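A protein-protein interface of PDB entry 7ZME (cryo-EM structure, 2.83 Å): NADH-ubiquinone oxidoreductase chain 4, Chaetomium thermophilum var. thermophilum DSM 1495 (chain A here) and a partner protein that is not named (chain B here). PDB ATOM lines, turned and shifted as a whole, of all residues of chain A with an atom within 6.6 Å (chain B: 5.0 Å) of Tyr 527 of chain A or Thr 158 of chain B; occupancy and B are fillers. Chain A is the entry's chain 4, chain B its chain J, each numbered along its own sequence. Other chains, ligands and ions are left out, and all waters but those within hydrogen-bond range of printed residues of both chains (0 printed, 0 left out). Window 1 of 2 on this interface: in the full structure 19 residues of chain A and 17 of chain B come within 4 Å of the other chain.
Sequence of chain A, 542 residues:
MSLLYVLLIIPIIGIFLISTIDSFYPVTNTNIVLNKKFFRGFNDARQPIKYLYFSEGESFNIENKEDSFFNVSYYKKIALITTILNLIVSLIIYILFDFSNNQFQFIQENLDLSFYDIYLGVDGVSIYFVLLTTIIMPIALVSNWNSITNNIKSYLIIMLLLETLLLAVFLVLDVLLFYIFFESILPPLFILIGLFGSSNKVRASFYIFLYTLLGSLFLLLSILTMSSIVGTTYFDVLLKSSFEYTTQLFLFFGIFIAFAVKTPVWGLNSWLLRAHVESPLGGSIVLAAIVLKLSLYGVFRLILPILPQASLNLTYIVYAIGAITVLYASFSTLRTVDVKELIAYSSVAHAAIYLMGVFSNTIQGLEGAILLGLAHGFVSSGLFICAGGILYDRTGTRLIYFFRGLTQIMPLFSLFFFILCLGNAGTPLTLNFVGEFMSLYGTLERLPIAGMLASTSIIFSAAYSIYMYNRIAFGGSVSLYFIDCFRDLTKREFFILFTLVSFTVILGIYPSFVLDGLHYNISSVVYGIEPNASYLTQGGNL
O of Tyr 527 of chain A is in hydrogen-bond range of ND2 of Asn 361 of chain A, 2.7 Å away.
The backbone carbonyl oxygen (O) of Gly 167 of chain B is in hydrogen-bond range of the backbone NH (N) of Ile 529 of chain A.
Of the printed residues of chain B, Leu 312 of chain A touches Ile 162 and Ile 168. Of chain B, only Thr 158, Ile 162 and Ile 168 come within 4 Å of Tyr 527 of chain A. Printed residues of chain B within 4 Å of Ile 529 of chain A: Gly 167. Thr 158 of chain B touches just one residue of chain A: Tyr 527 (3.7 Å). Of the printed residues of chain A, Ile 162 of chain B touches Gln 309, Leu 312 and Tyr 527. Printed residues of chain A within 4 Å of Ile 168 of chain B: Leu 312, Tyr 527 and Gly 528. The nearest residue of chain B that does not touch Tyr 527 of chain A is Gly 167 of chain B (4.5 Å). The nearest residue of chain A that does not touch Thr 158 of chain B is Gln 309 of chain A (4.1 Å).
Of the 12 printed residues of chain B, 4 touch a printed residue of chain A. Hydrophobic or aromatic side chains of chain B that line the printed part of chain A: Ile 162 and Ile 168. Among the printed residues, 9 pairs touch across the chains.
Among the printed residues, merely in contact across the chains: Gly 528 of chain A with Gly 167 of chain B (3.3 Å), Gln 309 of chain A with Ile 162 of chain B (3.4 Å), Tyr 527 of chain A with Thr 158 of chain B (3.7 Å), Gly 528 of chain A with Ile 168 of chain B (3.8 Å), Leu 312 of chain A with Ile 162 of chain B (3.9 Å), Leu 312 of chain A with Ile 168 of chain B (3.9 Å), Tyr 527 of chain A with Ile 168 of chain B (3.96 Å) and Tyr 527 of chain A with Ile 162 of chain B (3.97 Å).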
ATOM      1  N   LEU A 304      21.547  27.560  19.694  1.00  0.00           N
ATOM      2  CA  LEU A 304      20.672  26.620  18.933  1.00  0.00           C
ATOM      3  C   LEU A 304      19.977  27.232  17.711  1.00  0.00           C
ATOM      4  O   LEU A 304      20.023  26.577  16.661  1.00  0.00           O
ATOM      5  CB  LEU A 304      19.672  25.954  19.880  1.00  0.00           C
ATOM      6  CG  LEU A 304      20.301  25.278  21.093  1.00  0.00           C
ATOM      7  CD1 LEU A 304      19.235  24.698  22.006  1.00  0.00           C
ATOM      8  CD2 LEU A 304      21.301  24.217  20.666  1.00  0.00           C
ATOM      9  N   PRO A 308      23.138  26.238  13.961  1.00  0.00           N
ATOM     10  CA  PRO A 308      22.674  24.851  13.999  1.00  0.00           C
ATOM     11  C   PRO A 308      23.721  23.794  13.652  1.00  0.00           C
ATOM     12  O   PRO A 308      23.866  22.854  14.398  1.00  0.00           O
ATOM     13  CB  PRO A 308      21.640  24.871  12.879  1.00  0.00           C
ATOM     14  CG  PRO A 308      21.202  26.300  12.770  1.00  0.00           C
ATOM     15  CD  PRO A 308      22.515  27.025  12.899  1.00  0.00           C
ATOM     16  N   GLN A 309      24.453  24.009  12.564  1.00  0.00           N
ATOM     17  CA  GLN A 309      25.465  23.048  12.079  1.00  0.00           C
ATOM     18  C   GLN A 309      26.647  22.937  13.043  1.00  0.00           C
ATOM     19  O   GLN A 309      27.152  21.822  13.214  1.00  0.00           O
ATOM     20  CB  GLN A 309      25.840  23.519  10.684  1.00  0.00           C
ATOM     21  CG  GLN A 309      24.627  24.001   9.903  1.00  0.00           C
ATOM     22  CD  GLN A 309      24.940  24.407   8.488  1.00  0.00           C
ATOM     23  OE1 GLN A 309      25.930  23.978   7.901  1.00  0.00           O
ATOM     24  NE2 GLN A 309      24.081  25.234   7.920  1.00  0.00           N
ATOM     25  N   LEU A 312      25.785  20.905  16.036  1.00  0.00           N
ATOM     26  CA  LEU A 312      25.696  19.467  15.691  1.00  0.00           C
ATOM     27  C   LEU A 312      27.105  18.882  15.561  1.00  0.00           C
ATOM     28  O   LEU A 312      27.346  17.807  16.129  1.00  0.00           O
ATOM     29  CB  LEU A 312      24.926  19.342  14.376  1.00  0.00           C
ATOM     30  CG  LEU A 312      24.483  17.930  14.000  1.00  0.00           C
ATOM     31  CD1 LEU A 312      23.478  17.393  15.005  1.00  0.00           C
ATOM     32  CD2 LEU A 312      23.895  17.907  12.601  1.00  0.00           C
ATOM     33  N   ASN A 361      19.638  18.159  20.939  1.00  0.00           N
ATOM     34  CA  ASN A 361      18.865  18.301  19.674  1.00  0.00           C
ATOM     35  C   ASN A 361      17.634  17.410  19.815  1.00  0.00           C
ATOM     36  O   ASN A 361      17.123  16.922  18.799  1.00  0.00           O
ATOM     37  CB  ASN A 361      19.724  18.110  18.421  1.00  0.00           C
ATOM     38  CG  ASN A 361      19.180  18.803  17.195  1.00  0.00           C
ATOM     39  OD1 ASN A 361      18.384  19.727  17.301  1.00  0.00           O
ATOM     40  ND2 ASN A 361      19.623  18.368  16.031  1.00  0.00           N
ATOM     41  N   SER A 523       9.978  23.552  20.375  1.00  0.00           N
ATOM     42  CA  SER A 523       9.875  22.934  19.061  1.00  0.00           C
ATOM     43  C   SER A 523      10.584  23.756  17.993  1.00  0.00           C
ATOM     44  O   SER A 523      10.938  23.215  16.944  1.00  0.00           O
ATOM     45  CB  SER A 523       8.408  22.742  18.695  1.00  0.00           C
ATOM     46  OG  SER A 523       7.726  22.057  19.728  1.00  0.00           O
ATOM     47  N   VAL A 525      13.557  25.189  18.323  1.00  0.00           N
ATOM     48  CA  VAL A 525      15.003  25.191  18.501  1.00  0.00           C
ATOM     49  C   VAL A 525      15.624  23.841  18.173  1.00  0.00           C
ATOM     50  O   VAL A 525      16.802  23.624  18.453  1.00  0.00           O
ATOM     51  CB  VAL A 525      15.399  25.641  19.923  1.00  0.00           C
ATOM     52  CG1 VAL A 525      14.778  26.989  20.252  1.00  0.00           C
ATOM     53  CG2 VAL A 525      15.018  24.601  20.950  1.00  0.00           C
ATOM     54  N   VAL A 526      14.860  22.927  17.577  1.00  0.00           N
ATOM     55  CA  VAL A 526      15.382  21.637  17.143  1.00  0.00           C
ATOM     56  C   VAL A 526      15.856  21.769  15.703  1.00  0.00           C
ATOM     57  O   VAL A 526      15.335  22.579  14.933  1.00  0.00           O
ATOM     58  CB  VAL A 526      14.321  20.528  17.294  1.00  0.00           C
ATOM     59  CG1 VAL A 526      14.944  19.153  17.114  1.00  0.00           C
ATOM     60  CG2 VAL A 526      13.639  20.626  18.639  1.00  0.00           C
ATOM     61  N   TYR A 527      16.853  20.971  15.333  1.00  0.00           N
ATOM     62  CA  TYR A 527      17.463  21.026  14.007  1.00  0.00           C
ATOM     63  C   TYR A 527      17.428  19.632  13.394  1.00  0.00           C
ATOM     64  O   TYR A 527      18.168  18.741  13.823  1.00  0.00           O
ATOM     65  CB  TYR A 527      18.892  21.553  14.092  1.00  0.00           C
ATOM     66  CG  TYR A 527      19.511  21.885  12.758  1.00  0.00           C
ATOM     67  CD1 TYR A 527      18.941  22.834  11.923  1.00  0.00           C
ATOM     68  CD2 TYR A 527      20.670  21.249  12.334  1.00  0.00           C
ATOM     69  CE1 TYR A 527      19.507  23.140  10.704  1.00  0.00           C
ATOM     70  CE2 TYR A 527      21.243  21.548  11.122  1.00  0.00           C
ATOM     71  CZ  TYR A 527      20.660  22.494  10.310  1.00  0.00           C
ATOM     72  OH  TYR A 527      21.229  22.793   9.095  1.00  0.00           O
ATOM     73  N   GLY A 528      16.582  19.445  12.396  1.00  0.00           N
ATOM     74  CA  GLY A 528      16.482  18.164  11.729  1.00  0.00           C
ATOM     75  C   GLY A 528      15.166  18.029  11.004  1.00  0.00           C
ATOM     76  O   GLY A 528      14.246  18.826  11.175  1.00  0.00           O
ATOM     77  N   ILE A 529      15.098  16.993  10.170  1.00  0.00           N
ATOM     78  CA  ILE A 529      13.909  16.656   9.397  1.00  0.00           C
ATOM     79  C   ILE A 529      13.793  15.140   9.309  1.00  0.00           C
ATOM     80  O   ILE A 529      14.739  14.402   9.579  1.00  0.00           O
ATOM     81  CB  ILE A 529      13.920  17.268   7.976  1.00  0.00           C
ATOM     82  CG1 ILE A 529      15.104  16.734   7.168  1.00  0.00           C
ATOM     83  CG2 ILE A 529      13.874  18.788   8.011  1.00  0.00           C
ATOM     84  CD1 ILE A 529      15.048  17.103   5.704  1.00  0.00           C
ATOM     85  N   PRO B 154      20.854  25.508  -0.838  1.00  0.00           N
ATOM     86  CA  PRO B 154      20.499  24.159  -1.287  1.00  0.00           C
ATOM     87  C   PRO B 154      20.886  23.129  -0.242  1.00  0.00           C
ATOM     88  O   PRO B 154      21.886  23.277   0.464  1.00  0.00           O
ATOM     89  CB  PRO B 154      21.302  23.991  -2.582  1.00  0.00           C
ATOM     90  CG  PRO B 154      22.407  24.986  -2.478  1.00  0.00           C
ATOM     91  CD  PRO B 154      21.829  26.149  -1.737  1.00  0.00           C
ATOM     92  N   ILE B 155      20.068  22.079  -0.133  1.00  0.00           N
ATOM     93  CA  ILE B 155      20.293  21.078   0.898  1.00  0.00           C
ATOM     94  C   ILE B 155      21.619  20.361   0.697  1.00  0.00           C
ATOM     95  O   ILE B 155      22.192  19.842   1.657  1.00  0.00           O
ATOM     96  CB  ILE B 155      19.115  20.085   0.950  1.00  0.00           C
ATOM     97  CG1 ILE B 155      19.057  19.405   2.319  1.00  0.00           C
ATOM     98  CG2 ILE B 155      19.224  19.058  -0.160  1.00  0.00           C
ATOM     99  CD1 ILE B 155      17.874  18.500   2.507  1.00  0.00           C
ATOM    100  N   GLU B 156      22.134  20.332  -0.533  1.00  0.00           N
ATOM    101  CA  GLU B 156      23.402  19.659  -0.783  1.00  0.00           C
ATOM    102  C   GLU B 156      24.555  20.331  -0.050  1.00  0.00           C
ATOM    103  O   GLU B 156      25.539  19.669   0.295  1.00  0.00           O
ATOM    104  CB  GLU B 156      23.683  19.610  -2.285  1.00  0.00           C
ATOM    105  N   GLU B 157      24.457  21.638   0.201  1.00  0.00           N
ATOM    106  CA  GLU B 157      25.555  22.345   0.851  1.00  0.00           C
ATOM    107  C   GLU B 157      25.679  21.951   2.317  1.00  0.00           C
ATOM    108  O   GLU B 157      26.786  21.718   2.814  1.00  0.00           O
ATOM    109  CB  GLU B 157      25.365  23.856   0.709  1.00  0.00           C
ATOM    110  CG  GLU B 157      25.573  24.365  -0.707  1.00  0.00           C
ATOM    111  CD  GLU B 157      25.353  25.858  -0.828  1.00  0.00           C
ATOM    112  OE1 GLU B 157      24.880  26.472   0.151  1.00  0.00           O
ATOM    113  OE2 GLU B 157      25.657  26.420  -1.902  1.00  0.00           O
ATOM    114  N   THR B 158      24.556  21.883   3.033  1.00  0.00           N
ATOM    115  CA  THR B 158      24.605  21.433   4.419  1.00  0.00           C
ATOM    116  C   THR B 158      24.905  19.942   4.506  1.00  0.00           C
ATOM    117  O   THR B 158      25.710  19.514   5.341  1.00  0.00           O
ATOM    118  CB  THR B 158      23.297  21.765   5.140  1.00  0.00           C
ATOM    119  OG1 THR B 158      23.323  21.210   6.459  1.00  0.00           O
ATOM    120  CG2 THR B 158      22.105  21.202   4.405  1.00  0.00           C
ATOM    121  N   LEU B 159      24.286  19.134   3.643  1.00  0.00           N
ATOM    122  CA  LEU B 159      24.454  17.689   3.740  1.00  0.00           C
ATOM    123  C   LEU B 159      25.887  17.274   3.449  1.00  0.00           C
ATOM    124  O   LEU B 159      26.427  16.379   4.108  1.00  0.00           O
ATOM    125  CB  LEU B 159      23.489  16.978   2.793  1.00  0.00           C
ATOM    126  CG  LEU B 159      22.009  17.122   3.117  1.00  0.00           C
ATOM    127  CD1 LEU B 159      21.159  16.491   2.030  1.00  0.00           C
ATOM    128  CD2 LEU B 159      21.728  16.495   4.456  1.00  0.00           C
ATOM    129  N   ALA B 160      26.523  17.911   2.468  1.00  0.00           N
ATOM    130  CA  ALA B 160      27.888  17.538   2.139  1.00  0.00           C
ATOM    131  C   ALA B 160      28.873  17.923   3.227  1.00  0.00           C
ATOM    132  O   ALA B 160      30.018  17.459   3.194  1.00  0.00           O
ATOM    133  CB  ALA B 160      28.311  18.177   0.815  1.00  0.00           C
ATOM    134  N   GLU B 161      28.465  18.749   4.186  1.00  0.00           N
ATOM    135  CA  GLU B 161      29.411  19.329   5.115  1.00  0.00           C
ATOM    136  C   GLU B 161      28.917  19.362   6.562  1.00  0.00           C
ATOM    137  O   GLU B 161      29.654  19.830   7.437  1.00  0.00           O
ATOM    138  CB  GLU B 161      29.804  20.727   4.609  1.00  0.00           C
ATOM    139  CG  GLU B 161      31.047  21.349   5.194  1.00  0.00           C
ATOM    140  CD  GLU B 161      30.998  22.850   5.109  1.00  0.00           C
ATOM    141  OE1 GLU B 161      30.740  23.487   6.133  1.00  0.00           O
ATOM    142  OE2 GLU B 161      31.219  23.406   4.009  1.00  0.00           O
ATOM    143  N   ILE B 162      27.710  18.873   6.849  1.00  0.00           N
ATOM    144  CA  ILE B 162      27.378  18.384   8.185  1.00  0.00           C
ATOM    145  C   ILE B 162      27.053  16.903   8.186  1.00  0.00           C
ATOM    146  O   ILE B 162      26.829  16.335   9.268  1.00  0.00           O
ATOM    147  CB  ILE B 162      26.216  19.167   8.832  1.00  0.00           C
ATOM    148  CG1 ILE B 162      24.880  18.730   8.240  1.00  0.00           C
ATOM    149  CG2 ILE B 162      26.432  20.662   8.699  1.00  0.00           C
ATOM    150  CD1 ILE B 162      23.686  19.270   8.981  1.00  0.00           C
ATOM    151  N   GLY B 163      27.026  16.261   7.028  1.00  0.00           N
ATOM    152  CA  GLY B 163      26.728  14.855   6.939  1.00  0.00           C
ATOM    153  C   GLY B 163      25.239  14.575   6.896  1.00  0.00           C
ATOM    154  O   GLY B 163      24.395  15.470   6.854  1.00  0.00           O
ATOM    155  N   GLY B 167      19.786  12.894  13.237  1.00  0.00           N
ATOM    156  CA  GLY B 167      18.595  13.696  13.107  1.00  0.00           C
ATOM    157  C   GLY B 167      18.447  14.405  11.780  1.00  0.00           C
ATOM    158  O   GLY B 167      17.393  14.998  11.529  1.00  0.00           O
ATOM    159  N   ILE B 168      19.463  14.360  10.926  1.00  0.00           N
ATOM    160  CA  ILE B 168      19.394  14.919   9.582  1.00  0.00           C
ATOM    161  C   ILE B 168      19.021  13.768   8.658  1.00  0.00           C
ATOM    162  O   ILE B 168      19.878  13.000   8.213  1.00  0.00           O
ATOM    163  CB  ILE B 168      20.708  15.586   9.172  1.00  0.00           C
ATOM    164  CG1 ILE B 168      21.101  16.650  10.199  1.00  0.00           C
ATOM    165  CG2 ILE B 168      20.577  16.207   7.806  1.00  0.00           C
ATOM    166  CD1 ILE B 168      20.017  17.667  10.484  1.00  0.00           C
